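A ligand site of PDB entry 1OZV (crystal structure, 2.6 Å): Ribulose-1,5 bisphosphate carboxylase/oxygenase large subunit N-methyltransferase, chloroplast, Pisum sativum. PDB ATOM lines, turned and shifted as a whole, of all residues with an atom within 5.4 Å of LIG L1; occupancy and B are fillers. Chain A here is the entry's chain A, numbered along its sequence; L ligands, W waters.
S1 of LIG L1 sits close to O of Ser 177, 3.6 Å away. O of Asp 195 lies close to S1 of LIG L1 (3.6 Å). Residues that only touch LIG L1: Gly 37 (3.4 Å), Pro 107 (3.1 Å), Leu 196 (3.7 Å), Ile 197 (3.7 Å), Tyr 243 (3.2 Å), Tyr 256 (3.3 Å), Gly 257 (3.9 Å) and Phe 258 (3.7 Å). Of the 21 residues printed, 15 come within 4 Å of LIG L1. Along chain A the residues within 4 Å of LIG L1 span positions 36 to 258. The nearest printed residue that does not touch LIG L1 is Thr 110 (4.1 Å).
NH2 of Arg 178 is in salt-bridge range of O1 of LIG L1, at 2.5 Å. O2 of LIG L1 is in hydrogen-bond range of N of Leu 38, at 2.6 Å. O of Leu 38 sits at hydrogen-bond distance from N1 of LIG L1 (2.7 Å). The backbone NH (N) of His 199 lies within hydrogen-bond range of a nitrogen (N3) of LIG L1 (3.1 Å). The backbone carbonyl oxygen (O) of His 199 lies within hydrogen-bond range of a nitrogen (N4) of LIG L1. O of Glu 36 lies within hydrogen-bond range of N1 of LIG L1 (2.8 Å). The side-chain amide oxygen of Asn 198 sits at hydrogen-bond distance from a nitrogen (N1) of LIG L1, at 2.9 Å. The side-chain hydroxyl (OH) of Tyr 256 sits at hydrogen-bond distance from a nitrogen (N1) of LG2 L2, 2.9 Å away. The backbone carbonyl oxygen (O) of Asp 195 sits at hydrogen-bond distance from a nitrogen (N2) of LG2 L2.
OD2 of Asp 195 is in salt-bridge range of NE of Arg 178 (3.2 Å). The side-chain amide nitrogen (ND2) of Asn 198 lies within hydrogen-bond range of the backbone carbonyl oxygen (O) of Leu 38. A ring nitrogen (ND1) of His 199 sits at hydrogen-bond distance from the backbone NH (N) of Tyr 243. The backbone carbonyl oxygen (O) of Ile 197 lies within hydrogen-bond range of the side-chain hydroxyl (OH) of Tyr 243, at 2.7 Å.
Water W3 lies within hydrogen-bond range of the backbone NH of Asp 111 (2.5 Å), an oxygen (O5) of LIG L1 (2.7 Å) and the backbone NH of Gly 257 (3.4 Å). Water W5 lies within hydrogen-bond range of O1 of LIG L1 (2.8 Å), NH2 of Arg 178 (3.1 Å) and O of Ile 105 (3.3 Å). Water W4 bridges the backbone carbonyl oxygen (O) of Glu 36 (2.8 Å) and an oxygen (O3) of LIG L1 (3.1 Å).
A sulfur (S1) of LIG L1 lies close to a nitrogen (N2) of LG2 L2, 3.3 Å away.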
ATOM      1  N   GLU A  36     -22.312  12.090  -5.282  1.00  0.00           N
ATOM      2  CA  GLU A  36     -20.867  11.949  -5.213  1.00  0.00           C
ATOM      3  C   GLU A  36     -20.363  11.185  -3.981  1.00  0.00           C
ATOM      4  O   GLU A  36     -19.244  11.440  -3.520  1.00  0.00           O
ATOM      5  CB  GLU A  36     -20.197  13.323  -5.309  1.00  0.00           C
ATOM      6  CG  GLU A  36     -20.806  14.405  -4.451  1.00  0.00           C
ATOM      7  CD  GLU A  36     -21.937  15.170  -5.138  1.00  0.00           C
ATOM      8  OE1 GLU A  36     -21.649  16.108  -5.917  1.00  0.00           O
ATOM      9  OE2 GLU A  36     -23.119  14.829  -4.893  1.00  0.00           O
ATOM     10  N   GLY A  37     -21.169  10.256  -3.469  1.00  0.00           N
ATOM     11  CA  GLY A  37     -20.770   9.459  -2.315  1.00  0.00           C
ATOM     12  C   GLY A  37     -21.382   9.895  -0.996  1.00  0.00           C
ATOM     13  O   GLY A  37     -22.557   9.616  -0.708  1.00  0.00           O
ATOM     14  N   LEU A  38     -20.575  10.537  -0.159  1.00  0.00           N
ATOM     15  CA  LEU A  38     -21.029  11.073   1.126  1.00  0.00           C
ATOM     16  C   LEU A  38     -20.681  12.547   1.090  1.00  0.00           C
ATOM     17  O   LEU A  38     -19.674  12.936   0.497  1.00  0.00           O
ATOM     18  CB  LEU A  38     -20.320  10.407   2.302  1.00  0.00           C
ATOM     19  CG  LEU A  38     -20.710   8.965   2.631  1.00  0.00           C
ATOM     20  CD1 LEU A  38     -19.748   8.416   3.672  1.00  0.00           C
ATOM     21  CD2 LEU A  38     -22.148   8.899   3.135  1.00  0.00           C
ATOM     22  N   GLY A  39     -21.521  13.373   1.692  1.00  0.00           N
ATOM     23  CA  GLY A  39     -21.216  14.789   1.669  1.00  0.00           C
ATOM     24  C   GLY A  39     -21.738  15.482   2.901  1.00  0.00           C
ATOM     25  O   GLY A  39     -22.271  14.852   3.813  1.00  0.00           O
ATOM     26  N   ILE A 105     -15.959   4.203   7.344  1.00  0.00           N
ATOM     27  CA  ILE A 105     -16.759   5.130   6.543  1.00  0.00           C
ATOM     28  C   ILE A 105     -16.115   5.339   5.192  1.00  0.00           C
ATOM     29  O   ILE A 105     -16.817   5.574   4.207  1.00  0.00           O
ATOM     30  CB  ILE A 105     -16.902   6.483   7.277  1.00  0.00           C
ATOM     31  CG1 ILE A 105     -17.980   6.352   8.339  1.00  0.00           C
ATOM     32  CG2 ILE A 105     -17.224   7.606   6.302  1.00  0.00           C
ATOM     33  CD1 ILE A 105     -19.247   5.670   7.844  1.00  0.00           C
ATOM     34  N   PRO A 107     -14.447   5.055   1.548  1.00  0.00           N
ATOM     35  CA  PRO A 107     -14.760   4.314   0.320  1.00  0.00           C
ATOM     36  C   PRO A 107     -13.615   3.360   0.049  1.00  0.00           C
ATOM     37  O   PRO A 107     -12.442   3.746   0.148  1.00  0.00           O
ATOM     38  CB  PRO A 107     -14.836   5.411  -0.742  1.00  0.00           C
ATOM     39  CG  PRO A 107     -15.175   6.656   0.049  1.00  0.00           C
ATOM     40  CD  PRO A 107     -14.321   6.498   1.278  1.00  0.00           C
ATOM     41  N   THR A 110     -12.245   4.586  -5.543  1.00  0.00           N
ATOM     42  CA  THR A 110     -12.733   5.811  -6.176  1.00  0.00           C
ATOM     43  C   THR A 110     -12.630   5.524  -7.663  1.00  0.00           C
ATOM     44  O   THR A 110     -12.152   4.459  -8.063  1.00  0.00           O
ATOM     45  CB  THR A 110     -11.860   7.024  -5.859  1.00  0.00           C
ATOM     46  OG1 THR A 110     -10.606   6.899  -6.525  1.00  0.00           O
ATOM     47  CG2 THR A 110     -11.629   7.140  -4.360  1.00  0.00           C
ATOM     48  N   ASP A 111     -13.074   6.450  -8.508  1.00  0.00           N
ATOM     49  CA  ASP A 111     -12.977   6.217  -9.933  1.00  0.00           C
ATOM     50  C   ASP A 111     -11.671   6.728 -10.515  1.00  0.00           C
ATOM     51  O   ASP A 111     -11.564   6.970 -11.711  1.00  0.00           O
ATOM     52  CB  ASP A 111     -14.167   6.826 -10.678  1.00  0.00           C
ATOM     53  CG  ASP A 111     -15.445   6.043 -10.458  1.00  0.00           C
ATOM     54  OD1 ASP A 111     -15.339   4.795 -10.373  1.00  0.00           O
ATOM     55  OD2 ASP A 111     -16.530   6.650 -10.383  1.00  0.00           O
ATOM     56  N   SER A 177      -6.742  11.771  -2.879  1.00  0.00           N
ATOM     57  CA  SER A 177      -8.097  12.260  -3.107  1.00  0.00           C
ATOM     58  C   SER A 177      -8.740  12.861  -1.864  1.00  0.00           C
ATOM     59  O   SER A 177      -9.831  13.433  -1.927  1.00  0.00           O
ATOM     60  CB  SER A 177      -8.988  11.127  -3.652  1.00  0.00           C
ATOM     61  OG  SER A 177      -9.057  10.029  -2.756  1.00  0.00           O
ATOM     62  N   ARG A 178      -8.055  12.753  -0.729  1.00  0.00           N
ATOM     63  CA  ARG A 178      -8.603  13.275   0.509  1.00  0.00           C
ATOM     64  C   ARG A 178      -7.846  14.401   1.217  1.00  0.00           C
ATOM     65  O   ARG A 178      -8.437  15.413   1.588  1.00  0.00           O
ATOM     66  CB  ARG A 178      -8.810  12.124   1.491  1.00  0.00           C
ATOM     67  CG  ARG A 178      -9.869  11.158   1.040  1.00  0.00           C
ATOM     68  CD  ARG A 178     -10.211  10.204   2.162  1.00  0.00           C
ATOM     69  NE  ARG A 178     -11.463   9.502   1.905  1.00  0.00           N
ATOM     70  CZ  ARG A 178     -12.657  10.067   1.941  1.00  0.00           C
ATOM     71  NH1 ARG A 178     -12.798  11.349   2.214  1.00  0.00           N
ATOM     72  NH2 ARG A 178     -13.744   9.340   1.698  1.00  0.00           N
ATOM     73  N   ASP A 195     -13.392  15.876   5.683  1.00  0.00           N
ATOM     74  CA  ASP A 195     -12.907  14.962   4.669  1.00  0.00           C
ATOM     75  C   ASP A 195     -14.015  14.750   3.638  1.00  0.00           C
ATOM     76  O   ASP A 195     -13.773  14.685   2.445  1.00  0.00           O
ATOM     77  CB  ASP A 195     -12.535  13.635   5.344  1.00  0.00           C
ATOM     78  CG  ASP A 195     -11.583  12.800   4.520  1.00  0.00           C
ATOM     79  OD1 ASP A 195     -10.503  13.310   4.144  1.00  0.00           O
ATOM     80  OD2 ASP A 195     -11.907  11.619   4.266  1.00  0.00           O
ATOM     81  N   LEU A 196     -15.244  14.666   4.156  1.00  0.00           N
ATOM     82  CA  LEU A 196     -16.449  14.446   3.357  1.00  0.00           C
ATOM     83  C   LEU A 196     -16.886  15.605   2.459  1.00  0.00           C
ATOM     84  O   LEU A 196     -17.823  15.457   1.665  1.00  0.00           O
ATOM     85  CB  LEU A 196     -17.602  14.077   4.286  1.00  0.00           C
ATOM     86  CG  LEU A 196     -17.350  12.876   5.188  1.00  0.00           C
ATOM     87  CD1 LEU A 196     -18.457  12.782   6.209  1.00  0.00           C
ATOM     88  CD2 LEU A 196     -17.287  11.604   4.353  1.00  0.00           C
ATOM     89  N   ILE A 197     -16.229  16.758   2.575  1.00  0.00           N
ATOM     90  CA  ILE A 197     -16.570  17.927   1.761  1.00  0.00           C
ATOM     91  C   ILE A 197     -16.291  17.596   0.284  1.00  0.00           C
ATOM     92  O   ILE A 197     -15.200  17.136  -0.067  1.00  0.00           O
ATOM     93  CB  ILE A 197     -15.726  19.147   2.199  1.00  0.00           C
ATOM     94  CG1 ILE A 197     -16.246  20.427   1.552  1.00  0.00           C
ATOM     95  CG2 ILE A 197     -14.269  18.928   1.821  1.00  0.00           C
ATOM     96  CD1 ILE A 197     -17.528  20.925   2.147  1.00  0.00           C
ATOM     97  N   ASN A 198     -17.276  17.831  -0.588  1.00  0.00           N
ATOM     98  CA  ASN A 198     -17.099  17.544  -2.007  1.00  0.00           C
ATOM     99  C   ASN A 198     -16.726  18.753  -2.861  1.00  0.00           C
ATOM    100  O   ASN A 198     -16.699  19.899  -2.380  1.00  0.00           O
ATOM    101  CB  ASN A 198     -18.347  16.885  -2.583  1.00  0.00           C
ATOM    102  CG  ASN A 198     -18.466  15.421  -2.221  1.00  0.00           C
ATOM    103  OD1 ASN A 198     -17.499  14.675  -2.341  1.00  0.00           O
ATOM    104  ND2 ASN A 198     -19.638  15.018  -1.773  1.00  0.00           N
ATOM    105  N   HIS A 199     -16.449  18.485  -4.125  1.00  0.00           N
ATOM    106  CA  HIS A 199     -16.050  19.510  -5.074  1.00  0.00           C
ATOM    107  C   HIS A 199     -17.201  19.982  -5.964  1.00  0.00           C
ATOM    108  O   HIS A 199     -18.080  19.197  -6.324  1.00  0.00           O
ATOM    109  CB  HIS A 199     -14.913  18.980  -5.946  1.00  0.00           C
ATOM    110  CG  HIS A 199     -14.661  19.775  -7.186  1.00  0.00           C
ATOM    111  ND1 HIS A 199     -13.776  20.829  -7.225  1.00  0.00           N
ATOM    112  CD2 HIS A 199     -15.173  19.666  -8.435  1.00  0.00           C
ATOM    113  CE1 HIS A 199     -13.762  21.346  -8.444  1.00  0.00           C
ATOM    114  NE2 HIS A 199     -14.609  20.655  -9.198  1.00  0.00           N
ATOM    115  N   SER A 200     -17.191  21.266  -6.319  1.00  0.00           N
ATOM    116  CA  SER A 200     -18.213  21.812  -7.195  1.00  0.00           C
ATOM    117  C   SER A 200     -17.660  22.953  -8.042  1.00  0.00           C
ATOM    118  O   SER A 200     -16.879  23.774  -7.549  1.00  0.00           O
ATOM    119  CB  SER A 200     -19.410  22.312  -6.417  1.00  0.00           C
ATOM    120  OG  SER A 200     -20.357  22.879  -7.296  1.00  0.00           O
ATOM    121  N   TYR A 243     -11.708  22.076  -5.266  1.00  0.00           N
ATOM    122  CA  TYR A 243     -10.483  21.329  -5.032  1.00  0.00           C
ATOM    123  C   TYR A 243      -9.233  21.972  -5.648  1.00  0.00           C
ATOM    124  O   TYR A 243      -8.181  21.986  -5.027  1.00  0.00           O
ATOM    125  CB  TYR A 243     -10.615  19.878  -5.536  1.00  0.00           C
ATOM    126  CG  TYR A 243     -11.488  18.984  -4.684  1.00  0.00           C
ATOM    127  CD1 TYR A 243     -11.648  17.637  -5.002  1.00  0.00           C
ATOM    128  CD2 TYR A 243     -12.169  19.489  -3.574  1.00  0.00           C
ATOM    129  CE1 TYR A 243     -12.468  16.809  -4.232  1.00  0.00           C
ATOM    130  CE2 TYR A 243     -13.001  18.664  -2.796  1.00  0.00           C
ATOM    131  CZ  TYR A 243     -13.147  17.325  -3.132  1.00  0.00           C
ATOM    132  OH  TYR A 243     -13.934  16.507  -2.355  1.00  0.00           O
ATOM    133  N   ASP A 255      -6.353  12.352  -9.726  1.00  0.00           N
ATOM    134  CA  ASP A 255      -6.295  12.703  -8.309  1.00  0.00           C
ATOM    135  C   ASP A 255      -7.564  12.315  -7.577  1.00  0.00           C
ATOM    136  O   ASP A 255      -7.529  11.973  -6.405  1.00  0.00           O
ATOM    137  CB  ASP A 255      -6.018  14.179  -8.128  1.00  0.00           C
ATOM    138  CG  ASP A 255      -4.592  14.552  -8.494  1.00  0.00           C
ATOM    139  OD1 ASP A 255      -4.210  15.719  -8.290  1.00  0.00           O
ATOM    140  OD2 ASP A 255      -3.869  13.664  -9.003  1.00  0.00           O
ATOM    141  N   TYR A 256      -8.689  12.380  -8.277  1.00  0.00           N
ATOM    142  CA  TYR A 256      -9.983  11.982  -7.722  1.00  0.00           C
ATOM    143  C   TYR A 256     -10.599  11.214  -8.879  1.00  0.00           C
ATOM    144  O   TYR A 256      -9.983  11.100  -9.941  1.00  0.00           O
ATOM    145  CB  TYR A 256     -10.851  13.200  -7.387  1.00  0.00           C
ATOM    146  CG  TYR A 256     -10.046  14.391  -6.937  1.00  0.00           C
ATOM    147  CD1 TYR A 256      -9.634  15.366  -7.840  1.00  0.00           C
ATOM    148  CD2 TYR A 256      -9.628  14.526  -5.605  1.00  0.00           C
ATOM    149  CE1 TYR A 256      -8.827  16.419  -7.455  1.00  0.00           C
ATOM    150  CE2 TYR A 256      -8.805  15.583  -5.201  1.00  0.00           C
ATOM    151  CZ  TYR A 256      -8.418  16.528  -6.131  1.00  0.00           C
ATOM    152  OH  TYR A 256      -7.586  17.554  -5.765  1.00  0.00           O
ATOM    153  N   GLY A 257     -11.784  10.685  -8.710  1.00  0.00           N
ATOM    154  CA  GLY A 257     -12.341   9.956  -9.834  1.00  0.00           C
ATOM    155  C   GLY A 257     -13.327  10.787 -10.633  1.00  0.00           C
ATOM    156  O   GLY A 257     -14.422  10.293 -10.890  1.00  0.00           O
ATOM    157  N   PHE A 258     -12.982  12.019 -11.018  1.00  0.00           N
ATOM    158  CA  PHE A 258     -13.937  12.852 -11.757  1.00  0.00           C
ATOM    159  C   PHE A 258     -13.324  13.929 -12.643  1.00  0.00           C
ATOM    160  O   PHE A 258     -12.158  14.279 -12.491  1.00  0.00           O
ATOM    161  CB  PHE A 258     -14.939  13.501 -10.795  1.00  0.00           C
ATOM    162  CG  PHE A 258     -14.383  14.685 -10.029  1.00  0.00           C
ATOM    163  CD1 PHE A 258     -14.299  15.948 -10.627  1.00  0.00           C
ATOM    164  CD2 PHE A 258     -13.938  14.544  -8.721  1.00  0.00           C
ATOM    165  CE1 PHE A 258     -13.780  17.043  -9.938  1.00  0.00           C
ATOM    166  CE2 PHE A 258     -13.409  15.630  -8.017  1.00  0.00           C
ATOM    167  CZ  PHE A 258     -13.331  16.878  -8.632  1.00  0.00           C
HETATM  168  N1  LIG L   1     -17.762  11.985  -1.166  1.00  0.00           N
HETATM  169  C1  LIG L   1     -16.588  11.332  -0.570  1.00  0.00           C
HETATM  170  C2  LIG L   1     -15.813  12.355   0.312  1.00  0.00           C
HETATM  171  C3  LIG L   1     -15.050  13.408  -0.440  1.00  0.00           C
HETATM  172  S1  LIG L   1     -13.264  13.078  -0.768  1.00  0.00           S
HETATM  173  C4  LIG L   1     -17.006  10.058   0.240  1.00  0.00           C
HETATM  174  O1  LIG L   1     -16.168   9.493   0.983  1.00  0.00           O
HETATM  175  O2  LIG L   1     -18.160   9.599   0.154  1.00  0.00           O
HETATM  176  C5  LIG L   1     -13.263  13.345  -2.538  1.00  0.00           C
HETATM  177  C6  LIG L   1     -13.767  12.162  -3.342  1.00  0.00           C
HETATM  178  O3  LIG L   1     -15.220  12.213  -3.441  1.00  0.00           O
HETATM  179  C7  LIG L   1     -13.281  12.143  -4.784  1.00  0.00           C
HETATM  180  O4  LIG L   1     -12.069  11.405  -4.917  1.00  0.00           O
HETATM  181  C8  LIG L   1     -14.431  11.539  -5.566  1.00  0.00           C
HETATM  182  O5  LIG L   1     -14.455  10.134  -5.717  1.00  0.00           O
HETATM  183  C9  LIG L   1     -15.620  12.143  -4.805  1.00  0.00           C
HETATM  184  N2  LIG L   1     -16.017  13.477  -5.308  1.00  0.00           N
HETATM  185  C10 LIG L   1     -15.771  14.748  -4.782  1.00  0.00           C
HETATM  186  N3  LIG L   1     -16.260  15.735  -5.479  1.00  0.00           N
HETATM  187  C11 LIG L   1     -16.871  15.104  -6.550  1.00  0.00           C
HETATM  188  C12 LIG L   1     -17.608  15.596  -7.653  1.00  0.00           C
HETATM  189  N4  LIG L   1     -17.807  16.893  -7.873  1.00  0.00           N
HETATM  190  N5  LIG L   1     -18.107  14.691  -8.564  1.00  0.00           N
HETATM  191  C13 LIG L   1     -17.913  13.361  -8.357  1.00  0.00           C
HETATM  192  N6  LIG L   1     -17.235  12.772  -7.333  1.00  0.00           N
HETATM  193  C14 LIG L   1     -16.753  13.706  -6.448  1.00  0.00           C
HETATM  194  N1  LG2 L   2      -7.139  18.703  -3.116  1.00  0.00           N
HETATM  195  C1  LG2 L   2      -7.790  19.726  -2.245  1.00  0.00           C
HETATM  196  C2  LG2 L   2      -6.740  20.676  -1.701  1.00  0.00           C
HETATM  197  O1  LG2 L   2      -5.610  20.655  -2.245  1.00  0.00           O
HETATM  198  C3  LG2 L   2      -8.515  19.054  -1.078  1.00  0.00           C
HETATM  199  C4  LG2 L   2      -9.464  17.946  -1.472  1.00  0.00           C
HETATM  200  C5  LG2 L   2     -10.199  17.397  -0.257  1.00  0.00           C
HETATM  201  C6  LG2 L   2     -11.020  16.167  -0.608  1.00  0.00           C
HETATM  202  N2  LG2 L   2     -11.907  15.752   0.522  1.00  0.00           N
HETATM  203  O2  LG2 L   2      -7.053  21.430  -0.752  1.00  0.00           O
HETATM  204  O   HOH W   1     -17.746  10.102  -6.672  1.00  0.00           O
HETATM  205  O   HOH W   2     -14.522   8.846  -3.296  1.00  0.00           O
HETATM  206  O   HOH W   3     -14.341   8.554  -7.930  1.00  0.00           O
HETATM  207  O   HOH W   4     -17.071   9.714  -3.549  1.00  0.00           O
HETATM  208  O   HOH W   5     -15.990   8.686   3.695  1.00  0.00           O
HETATM  209  O   HOH W   6     -18.493   6.779  -1.032  1.00  0.00           O
